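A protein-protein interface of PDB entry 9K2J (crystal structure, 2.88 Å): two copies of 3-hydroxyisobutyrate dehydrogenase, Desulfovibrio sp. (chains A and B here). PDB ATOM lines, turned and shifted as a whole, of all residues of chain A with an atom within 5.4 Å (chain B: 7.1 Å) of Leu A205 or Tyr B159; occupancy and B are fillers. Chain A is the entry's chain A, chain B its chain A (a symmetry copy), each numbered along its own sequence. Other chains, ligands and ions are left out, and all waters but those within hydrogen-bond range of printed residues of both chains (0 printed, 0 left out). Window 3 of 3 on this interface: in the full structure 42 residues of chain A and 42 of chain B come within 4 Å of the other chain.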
ATOM      1  N   SER A 200      23.354 -10.138  28.268  1.00  0.00           N
ATOM      2  CA  SER A 200      22.420 -11.046  27.586  1.00  0.00           C
ATOM      3  C   SER A 200      22.970 -11.566  26.248  1.00  0.00           C
ATOM      4  O   SER A 200      23.173 -12.777  26.062  1.00  0.00           O
ATOM      5  CB  SER A 200      21.103 -10.288  27.404  1.00  0.00           C
ATOM      6  OG  SER A 200      20.685  -9.770  28.653  1.00  0.00           O
ATOM      7  N   GLN A 201      23.252 -10.627  25.330  1.00  0.00           N
ATOM      8  CA  GLN A 201      23.832 -10.911  24.025  1.00  0.00           C
ATOM      9  C   GLN A 201      25.170 -11.598  24.124  1.00  0.00           C
ATOM     10  O   GLN A 201      25.448 -12.512  23.339  1.00  0.00           O
ATOM     11  CB  GLN A 201      23.945  -9.606  23.217  1.00  0.00           C
ATOM     12  CG  GLN A 201      25.227  -9.519  22.267  1.00  0.00           C
ATOM     13  CD  GLN A 201      25.044  -8.517  21.108  1.00  0.00           C
ATOM     14  OE1 GLN A 201      23.976  -8.088  20.840  1.00  0.00           O
ATOM     15  NE2 GLN A 201      26.160  -7.985  20.581  1.00  0.00           N
ATOM     16  N   LEU A 202      26.034 -11.159  25.038  1.00  0.00           N
ATOM     17  CA  LEU A 202      27.304 -11.852  25.142  1.00  0.00           C
ATOM     18  C   LEU A 202      27.084 -13.322  25.471  1.00  0.00           C
ATOM     19  O   LEU A 202      27.677 -14.191  24.824  1.00  0.00           O
ATOM     20  CB  LEU A 202      28.194 -11.207  26.190  1.00  0.00           C
ATOM     21  CG  LEU A 202      29.594 -11.847  26.140  1.00  0.00           C
ATOM     22  CD1 LEU A 202      30.433 -11.376  24.953  1.00  0.00           C
ATOM     23  CD2 LEU A 202      30.360 -11.644  27.459  1.00  0.00           C
ATOM     24  N   LEU A 203      26.204 -13.621  26.442  1.00  0.00           N
ATOM     25  CA  LEU A 203      25.899 -15.010  26.779  1.00  0.00           C
ATOM     26  C   LEU A 203      25.309 -15.751  25.594  1.00  0.00           C
ATOM     27  O   LEU A 203      25.710 -16.887  25.301  1.00  0.00           O
ATOM     28  CB  LEU A 203      24.929 -15.085  27.954  1.00  0.00           C
ATOM     29  CG  LEU A 203      25.361 -15.265  29.410  1.00  0.00           C
ATOM     30  CD1 LEU A 203      26.063 -16.589  29.579  1.00  0.00           C
ATOM     31  CD2 LEU A 203      26.232 -14.146  29.879  1.00  0.00           C
ATOM     32  N   THR A 204      24.344 -15.135  24.909  1.00  0.00           N
ATOM     33  CA  THR A 204      23.709 -15.837  23.800  1.00  0.00           C
ATOM     34  C   THR A 204      24.754 -16.235  22.773  1.00  0.00           C
ATOM     35  O   THR A 204      24.737 -17.361  22.256  1.00  0.00           O
ATOM     36  CB  THR A 204      22.628 -14.973  23.150  1.00  0.00           C
ATOM     37  OG1 THR A 204      21.724 -14.494  24.149  1.00  0.00           O
ATOM     38  CG2 THR A 204      21.821 -15.844  22.203  1.00  0.00           C
ATOM     39  N   LEU A 205      25.712 -15.338  22.519  1.00  0.00           N
ATOM     40  CA  LEU A 205      26.730 -15.602  21.511  1.00  0.00           C
ATOM     41  C   LEU A 205      27.734 -16.637  21.996  1.00  0.00           C
ATOM     42  O   LEU A 205      28.100 -17.548  21.246  1.00  0.00           O
ATOM     43  CB  LEU A 205      27.456 -14.312  21.145  1.00  0.00           C
ATOM     44  CG  LEU A 205      26.625 -13.295  20.364  1.00  0.00           C
ATOM     45  CD1 LEU A 205      27.344 -11.967  20.261  1.00  0.00           C
ATOM     46  CD2 LEU A 205      26.291 -13.851  19.004  1.00  0.00           C
ATOM     47  N   LEU A 206      28.151 -16.551  23.262  1.00  0.00           N
ATOM     48  CA  LEU A 206      29.198 -17.443  23.744  1.00  0.00           C
ATOM     49  C   LEU A 206      28.682 -18.852  23.899  1.00  0.00           C
ATOM     50  O   LEU A 206      29.485 -19.791  23.936  1.00  0.00           O
ATOM     51  CB  LEU A 206      29.757 -16.953  25.071  1.00  0.00           C
ATOM     52  CG  LEU A 206      30.565 -15.654  25.033  1.00  0.00           C
ATOM     53  CD1 LEU A 206      31.134 -15.285  26.408  1.00  0.00           C
ATOM     54  CD2 LEU A 206      31.671 -15.727  23.962  1.00  0.00           C
ATOM     55  N   GLN A 207      27.357 -19.003  23.990  1.00  0.00           N
ATOM     56  CA  GLN A 207      26.752 -20.318  24.167  1.00  0.00           C
ATOM     57  C   GLN A 207      27.170 -21.290  23.061  1.00  0.00           C
ATOM     58  O   GLN A 207      27.427 -22.469  23.329  1.00  0.00           O
ATOM     59  CB  GLN A 207      25.234 -20.144  24.203  1.00  0.00           C
ATOM     60  CG  GLN A 207      24.385 -21.324  24.635  1.00  0.00           C
ATOM     61  CD  GLN A 207      22.968 -21.215  24.061  1.00  0.00           C
ATOM     62  OE1 GLN A 207      22.026 -20.812  24.764  1.00  0.00           O
ATOM     63  NE2 GLN A 207      22.820 -21.536  22.764  1.00  0.00           N
ATOM     64  N   ASP A 208      27.280 -20.816  21.821  1.00  0.00           N
ATOM     65  CA  ASP A 208      27.682 -21.682  20.714  1.00  0.00           C
ATOM     66  C   ASP A 208      29.178 -21.589  20.417  1.00  0.00           C
ATOM     67  O   ASP A 208      29.588 -21.631  19.253  1.00  0.00           O
ATOM     68  CB  ASP A 208      26.849 -21.364  19.470  1.00  0.00           C
ATOM     69  CG  ASP A 208      26.906 -22.481  18.404  1.00  0.00           C
ATOM     70  OD1 ASP A 208      26.471 -23.630  18.677  1.00  0.00           O
ATOM     71  OD2 ASP A 208      27.366 -22.199  17.277  1.00  0.00           O
ATOM     72  N   THR A 209      30.022 -21.465  21.443  1.00  0.00           N
ATOM     73  CA  THR A 209      31.467 -21.451  21.256  1.00  0.00           C
ATOM     74  C   THR A 209      32.104 -22.431  22.227  1.00  0.00           C
ATOM     75  O   THR A 209      31.423 -23.102  23.004  1.00  0.00           O
ATOM     76  CB  THR A 209      32.097 -20.064  21.463  1.00  0.00           C
ATOM     77  OG1 THR A 209      32.181 -19.785  22.863  1.00  0.00           O
ATOM     78  CG2 THR A 209      31.309 -18.967  20.756  1.00  0.00           C
ATOM     79  N   GLN B 118      34.319  -4.750  10.641  1.00  0.00           N
ATOM     80  CA  GLN B 118      35.043  -5.837  11.276  1.00  0.00           C
ATOM     81  C   GLN B 118      34.210  -7.091  11.179  1.00  0.00           C
ATOM     82  O   GLN B 118      32.999  -7.056  11.390  1.00  0.00           O
ATOM     83  CB  GLN B 118      35.305  -5.575  12.747  1.00  0.00           C
ATOM     84  CG  GLN B 118      36.294  -6.538  13.344  1.00  0.00           C
ATOM     85  CD  GLN B 118      37.684  -6.231  12.869  1.00  0.00           C
ATOM     86  OE1 GLN B 118      38.038  -5.066  12.718  1.00  0.00           O
ATOM     87  NE2 GLN B 118      38.475  -7.265  12.601  1.00  0.00           N
ATOM     88  N   CYS B 119      34.854  -8.199  10.894  1.00  0.00           N
ATOM     89  CA  CYS B 119      34.090  -9.404  10.695  1.00  0.00           C
ATOM     90  C   CYS B 119      34.916 -10.568  11.229  1.00  0.00           C
ATOM     91  O   CYS B 119      35.534 -11.310  10.463  1.00  0.00           O
ATOM     92  CB  CYS B 119      33.755  -9.596   9.223  1.00  0.00           C
ATOM     93  SG  CYS B 119      32.655 -10.913   8.967  1.00  0.00           S
ATOM     94  N   PRO B 134      30.462 -18.839  12.608  1.00  0.00           N
ATOM     95  CA  PRO B 134      29.739 -17.591  12.862  1.00  0.00           C
ATOM     96  C   PRO B 134      30.537 -16.399  12.362  1.00  0.00           C
ATOM     97  O   PRO B 134      31.772 -16.409  12.347  1.00  0.00           O
ATOM     98  CB  PRO B 134      29.609 -17.553  14.389  1.00  0.00           C
ATOM     99  CG  PRO B 134      30.017 -18.902  14.862  1.00  0.00           C
ATOM    100  CD  PRO B 134      30.980 -19.416  13.856  1.00  0.00           C
ATOM    101  N   LEU B 135      29.819 -15.369  11.917  1.00  0.00           N
ATOM    102  CA  LEU B 135      30.436 -14.086  11.596  1.00  0.00           C
ATOM    103  C   LEU B 135      29.981 -13.070  12.634  1.00  0.00           C
ATOM    104  O   LEU B 135      28.774 -12.878  12.825  1.00  0.00           O
ATOM    105  CB  LEU B 135      30.059 -13.594  10.200  1.00  0.00           C
ATOM    106  CG  LEU B 135      30.117 -14.525   9.006  1.00  0.00           C
ATOM    107  CD1 LEU B 135      29.537 -13.829   7.790  1.00  0.00           C
ATOM    108  CD2 LEU B 135      31.513 -14.984   8.755  1.00  0.00           C
ATOM    109  N   PHE B 136      30.938 -12.418  13.294  1.00  0.00           N
ATOM    110  CA  PHE B 136      30.655 -11.310  14.205  1.00  0.00           C
ATOM    111  C   PHE B 136      31.029 -10.032  13.463  1.00  0.00           C
ATOM    112  O   PHE B 136      32.211  -9.688  13.362  1.00  0.00           O
ATOM    113  CB  PHE B 136      31.424 -11.477  15.508  1.00  0.00           C
ATOM    114  CG  PHE B 136      31.295 -12.850  16.092  1.00  0.00           C
ATOM    115  CD1 PHE B 136      30.072 -13.284  16.603  1.00  0.00           C
ATOM    116  CD2 PHE B 136      32.374 -13.721  16.116  1.00  0.00           C
ATOM    117  CE1 PHE B 136      29.935 -14.559  17.132  1.00  0.00           C
ATOM    118  CE2 PHE B 136      32.243 -15.001  16.648  1.00  0.00           C
ATOM    119  CZ  PHE B 136      31.029 -15.421  17.151  1.00  0.00           C
ATOM    120  N   ILE B 137      30.022  -9.374  12.877  1.00  0.00           N
ATOM    121  CA  ILE B 137      30.216  -8.169  12.081  1.00  0.00           C
ATOM    122  C   ILE B 137      29.917  -6.960  12.949  1.00  0.00           C
ATOM    123  O   ILE B 137      28.867  -6.890  13.609  1.00  0.00           O
ATOM    124  CB  ILE B 137      29.334  -8.142  10.820  1.00  0.00           C
ATOM    125  CG1 ILE B 137      29.670  -9.247   9.817  1.00  0.00           C
ATOM    126  CG2 ILE B 137      29.461  -6.801  10.144  1.00  0.00           C
ATOM    127  CD1 ILE B 137      28.739 -10.407   9.836  1.00  0.00           C
ATOM    128  N   GLY B 138      30.861  -6.022  12.969  1.00  0.00           N
ATOM    129  CA  GLY B 138      30.655  -4.740  13.597  1.00  0.00           C
ATOM    130  C   GLY B 138      31.016  -3.634  12.627  1.00  0.00           C
ATOM    131  O   GLY B 138      31.773  -3.829  11.682  1.00  0.00           O
ATOM    132  N   PHE B 144      26.600  -3.444   6.663  1.00  0.00           N
ATOM    133  CA  PHE B 144      26.118  -4.789   6.975  1.00  0.00           C
ATOM    134  C   PHE B 144      24.803  -5.088   6.271  1.00  0.00           C
ATOM    135  O   PHE B 144      24.609  -6.196   5.757  1.00  0.00           O
ATOM    136  CB  PHE B 144      25.950  -4.958   8.486  1.00  0.00           C
ATOM    137  CG  PHE B 144      25.213  -6.210   8.876  1.00  0.00           C
ATOM    138  CD1 PHE B 144      25.884  -7.420   8.980  1.00  0.00           C
ATOM    139  CD2 PHE B 144      23.855  -6.182   9.154  1.00  0.00           C
ATOM    140  CE1 PHE B 144      25.209  -8.584   9.345  1.00  0.00           C
ATOM    141  CE2 PHE B 144      23.177  -7.345   9.511  1.00  0.00           C
ATOM    142  CZ  PHE B 144      23.855  -8.544   9.607  1.00  0.00           C
ATOM    143  N   SER B 156      27.818 -18.645   8.608  1.00  0.00           N
ATOM    144  CA  SER B 156      26.909 -19.463   9.456  1.00  0.00           C
ATOM    145  C   SER B 156      25.731 -18.588   9.875  1.00  0.00           C
ATOM    146  O   SER B 156      24.854 -18.445   9.030  1.00  0.00           O
ATOM    147  CB  SER B 156      27.713 -20.014  10.642  1.00  0.00           C
ATOM    148  OG  SER B 156      27.009 -20.982  11.382  1.00  0.00           O
ATOM    149  N   PRO B 157      25.624 -17.950  11.145  1.00  0.00           N
ATOM    150  CA  PRO B 157      24.695 -16.823  11.246  1.00  0.00           C
ATOM    151  C   PRO B 157      25.480 -15.542  11.094  1.00  0.00           C
ATOM    152  O   PRO B 157      26.648 -15.448  11.482  1.00  0.00           O
ATOM    153  CB  PRO B 157      24.061 -16.987  12.616  1.00  0.00           C
ATOM    154  CG  PRO B 157      24.877 -17.945  13.347  1.00  0.00           C
ATOM    155  CD  PRO B 157      26.061 -18.320  12.503  1.00  0.00           C
ATOM    156  N   ALA B 158      24.872 -14.543  10.471  1.00  0.00           N
ATOM    157  CA  ALA B 158      25.536 -13.247  10.357  1.00  0.00           C
ATOM    158  C   ALA B 158      25.083 -12.410  11.543  1.00  0.00           C
ATOM    159  O   ALA B 158      24.041 -11.755  11.505  1.00  0.00           O
ATOM    160  CB  ALA B 158      25.218 -12.591   9.025  1.00  0.00           C
ATOM    161  N   TYR B 159      25.877 -12.455  12.615  1.00  0.00           N
ATOM    162  CA  TYR B 159      25.579 -11.713  13.828  1.00  0.00           C
ATOM    163  C   TYR B 159      26.043 -10.278  13.637  1.00  0.00           C
ATOM    164  O   TYR B 159      27.175 -10.046  13.201  1.00  0.00           O
ATOM    165  CB  TYR B 159      26.302 -12.323  15.022  1.00  0.00           C
ATOM    166  CG  TYR B 159      25.802 -13.671  15.477  1.00  0.00           C
ATOM    167  CD1 TYR B 159      24.484 -13.846  15.909  1.00  0.00           C
ATOM    168  CD2 TYR B 159      26.659 -14.766  15.536  1.00  0.00           C
ATOM    169  CE1 TYR B 159      24.027 -15.083  16.354  1.00  0.00           C
ATOM    170  CE2 TYR B 159      26.212 -16.009  15.985  1.00  0.00           C
ATOM    171  CZ  TYR B 159      24.898 -16.155  16.389  1.00  0.00           C
ATOM    172  OH  TYR B 159      24.463 -17.369  16.835  1.00  0.00           O
ATOM    173  N   TYR B 160      25.171  -9.311  13.939  1.00  0.00           N
ATOM    174  CA  TYR B 160      25.525  -7.894  13.867  1.00  0.00           C
ATOM    175  C   TYR B 160      25.856  -7.392  15.269  1.00  0.00           C
ATOM    176  O   TYR B 160      24.975  -7.315  16.129  1.00  0.00           O
ATOM    177  CB  TYR B 160      24.405  -7.062  13.250  1.00  0.00           C
ATOM    178  CG  TYR B 160      24.766  -5.596  13.260  1.00  0.00           C
ATOM    179  CD1 TYR B 160      25.886  -5.145  12.572  1.00  0.00           C
ATOM    180  CD2 TYR B 160      24.034  -4.671  13.994  1.00  0.00           C
ATOM    181  CE1 TYR B 160      26.256  -3.812  12.583  1.00  0.00           C
ATOM    182  CE2 TYR B 160      24.396  -3.331  14.018  1.00  0.00           C
ATOM    183  CZ  TYR B 160      25.511  -2.906  13.305  1.00  0.00           C
ATOM    184  OH  TYR B 160      25.909  -1.579  13.301  1.00  0.00           O
ATOM    185  N   MET B 161      27.125  -7.051  15.504  1.00  0.00           N
ATOM    186  CA  MET B 161      27.581  -6.642  16.835  1.00  0.00           C
ATOM    187  C   MET B 161      27.408  -5.151  17.114  1.00  0.00           C
ATOM    188  O   MET B 161      27.679  -4.718  18.244  1.00  0.00           O
ATOM    189  CB  MET B 161      29.056  -7.018  17.048  1.00  0.00           C
ATOM    190  CG  MET B 161      29.347  -8.495  16.837  1.00  0.00           C
ATOM    191  SD  MET B 161      28.556  -9.575  18.052  1.00  0.00           S
ATOM    192  CE  MET B 161      28.957  -8.699  19.554  1.00  0.00           C
ATOM    193  N   GLY B 162      27.020  -4.349  16.123  1.00  0.00           N
ATOM    194  CA  GLY B 162      26.966  -2.915  16.349  1.00  0.00           C
ATOM    195  C   GLY B 162      28.294  -2.209  16.140  1.00  0.00           C
ATOM    196  O   GLY B 162      28.605  -1.788  15.015  1.00  0.00           O
ATOM    197  N   ALA B 166      33.058  -4.198  19.680  1.00  0.00           N
ATOM    198  CA  ALA B 166      32.295  -5.376  20.074  1.00  0.00           C
ATOM    199  C   ALA B 166      32.672  -6.578  19.222  1.00  0.00           C
ATOM    200  O   ALA B 166      32.823  -7.693  19.741  1.00  0.00           O
ATOM    201  CB  ALA B 166      30.800  -5.086  19.953  1.00  0.00           C
ATOM    202  N   SER B 167      32.833  -6.372  17.912  1.00  0.00           N
ATOM    203  CA  SER B 167      33.210  -7.473  17.031  1.00  0.00           C
ATOM    204  C   SER B 167      34.543  -8.087  17.429  1.00  0.00           C
ATOM    205  O   SER B 167      34.672  -9.314  17.498  1.00  0.00           O
ATOM    206  CB  SER B 167      33.255  -7.021  15.590  1.00  0.00           C
ATOM    207  OG  SER B 167      33.308  -8.174  14.779  1.00  0.00           O
ATOM    208  N   VAL B 170      34.073  -9.896  21.181  1.00  0.00           N
ATOM    209  CA  VAL B 170      33.389 -11.161  21.383  1.00  0.00           C
ATOM    210  C   VAL B 170      34.284 -12.321  20.942  1.00  0.00           C
ATOM    211  O   VAL B 170      34.362 -13.345  21.638  1.00  0.00           O
ATOM    212  CB  VAL B 170      32.005 -11.150  20.709  1.00  0.00           C
ATOM    213  CG1 VAL B 170      32.107 -11.052  19.219  1.00  0.00           C
ATOM    214  CG2 VAL B 170      31.237 -12.374  21.109  1.00  0.00           C
ATOM    215  N   SER B 174      35.687 -15.071  23.658  1.00  0.00           N
ATOM    216  CA  SER B 174      35.413 -16.494  23.534  1.00  0.00           C
ATOM    217  C   SER B 174      36.711 -17.282  23.613  1.00  0.00           C
ATOM    218  O   SER B 174      36.776 -18.320  24.286  1.00  0.00           O
ATOM    219  CB  SER B 174      34.625 -16.793  22.264  1.00  0.00           C
ATOM    220  OG  SER B 174      35.475 -16.800  21.158  1.00  0.00           O
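Among the printed residues, merely in contact across the chains: Gln A201 with Met B161, Leu A205 with Met B161, Leu A205 with Tyr B159, Leu A206 with Ser B174 and Thr A209 with Ser B174.
Along chain A the printed residues that touch a printed residue of chain B span positions 201 to 209.
Of the 19 printed residues of chain B, 3 touch a printed residue of chain A.
Among the printed residues, 5 pairs touch across the chains.
Among the printed residues, no Asp or Glu carboxylate lies within 4 Å of a Lys or Arg side-chain nitrogen of the other chain.
The backbone carbonyl oxygen (O) of Leu A206 sits at hydrogen-bond distance from the side-chain hydroxyl (OG1) of Thr A209 (2.9 Å).
The backbone NH (N) of Tyr B159 is in hydrogen-bond range of the backbone carbonyl oxygen (O) of Leu B135 (2.9 Å).
N of Ile B137 is in hydrogen-bond range of O of Tyr B159, at 2.9 Å.
O of Ile B137 sits at hydrogen-bond distance from N of Met B161 (2.6 Å).
No position is printed for both chains.
Of the 5 pairs that touch across the chains among the printed residues, none has its exchanged pair printed and touching as well.
Of the printed residues of chain B, Leu A206 touches Ser B174 (3.6 Å).
Of the printed residues of chain B, Thr A209 touches Ser B174.
Tyr B159 touches one residue of chain A.
Printed residues of chain A within 4 Å of Met B161: Gln A201 (3.1 Å) and Leu A205 (3.5 Å).
The nearest residue of chain A that does not touch Tyr B159 is Asp A208 (5.3 Å).
The nearest printed residue of chain B that does not touch Thr A209 is Phe B136 (5.1 Å).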
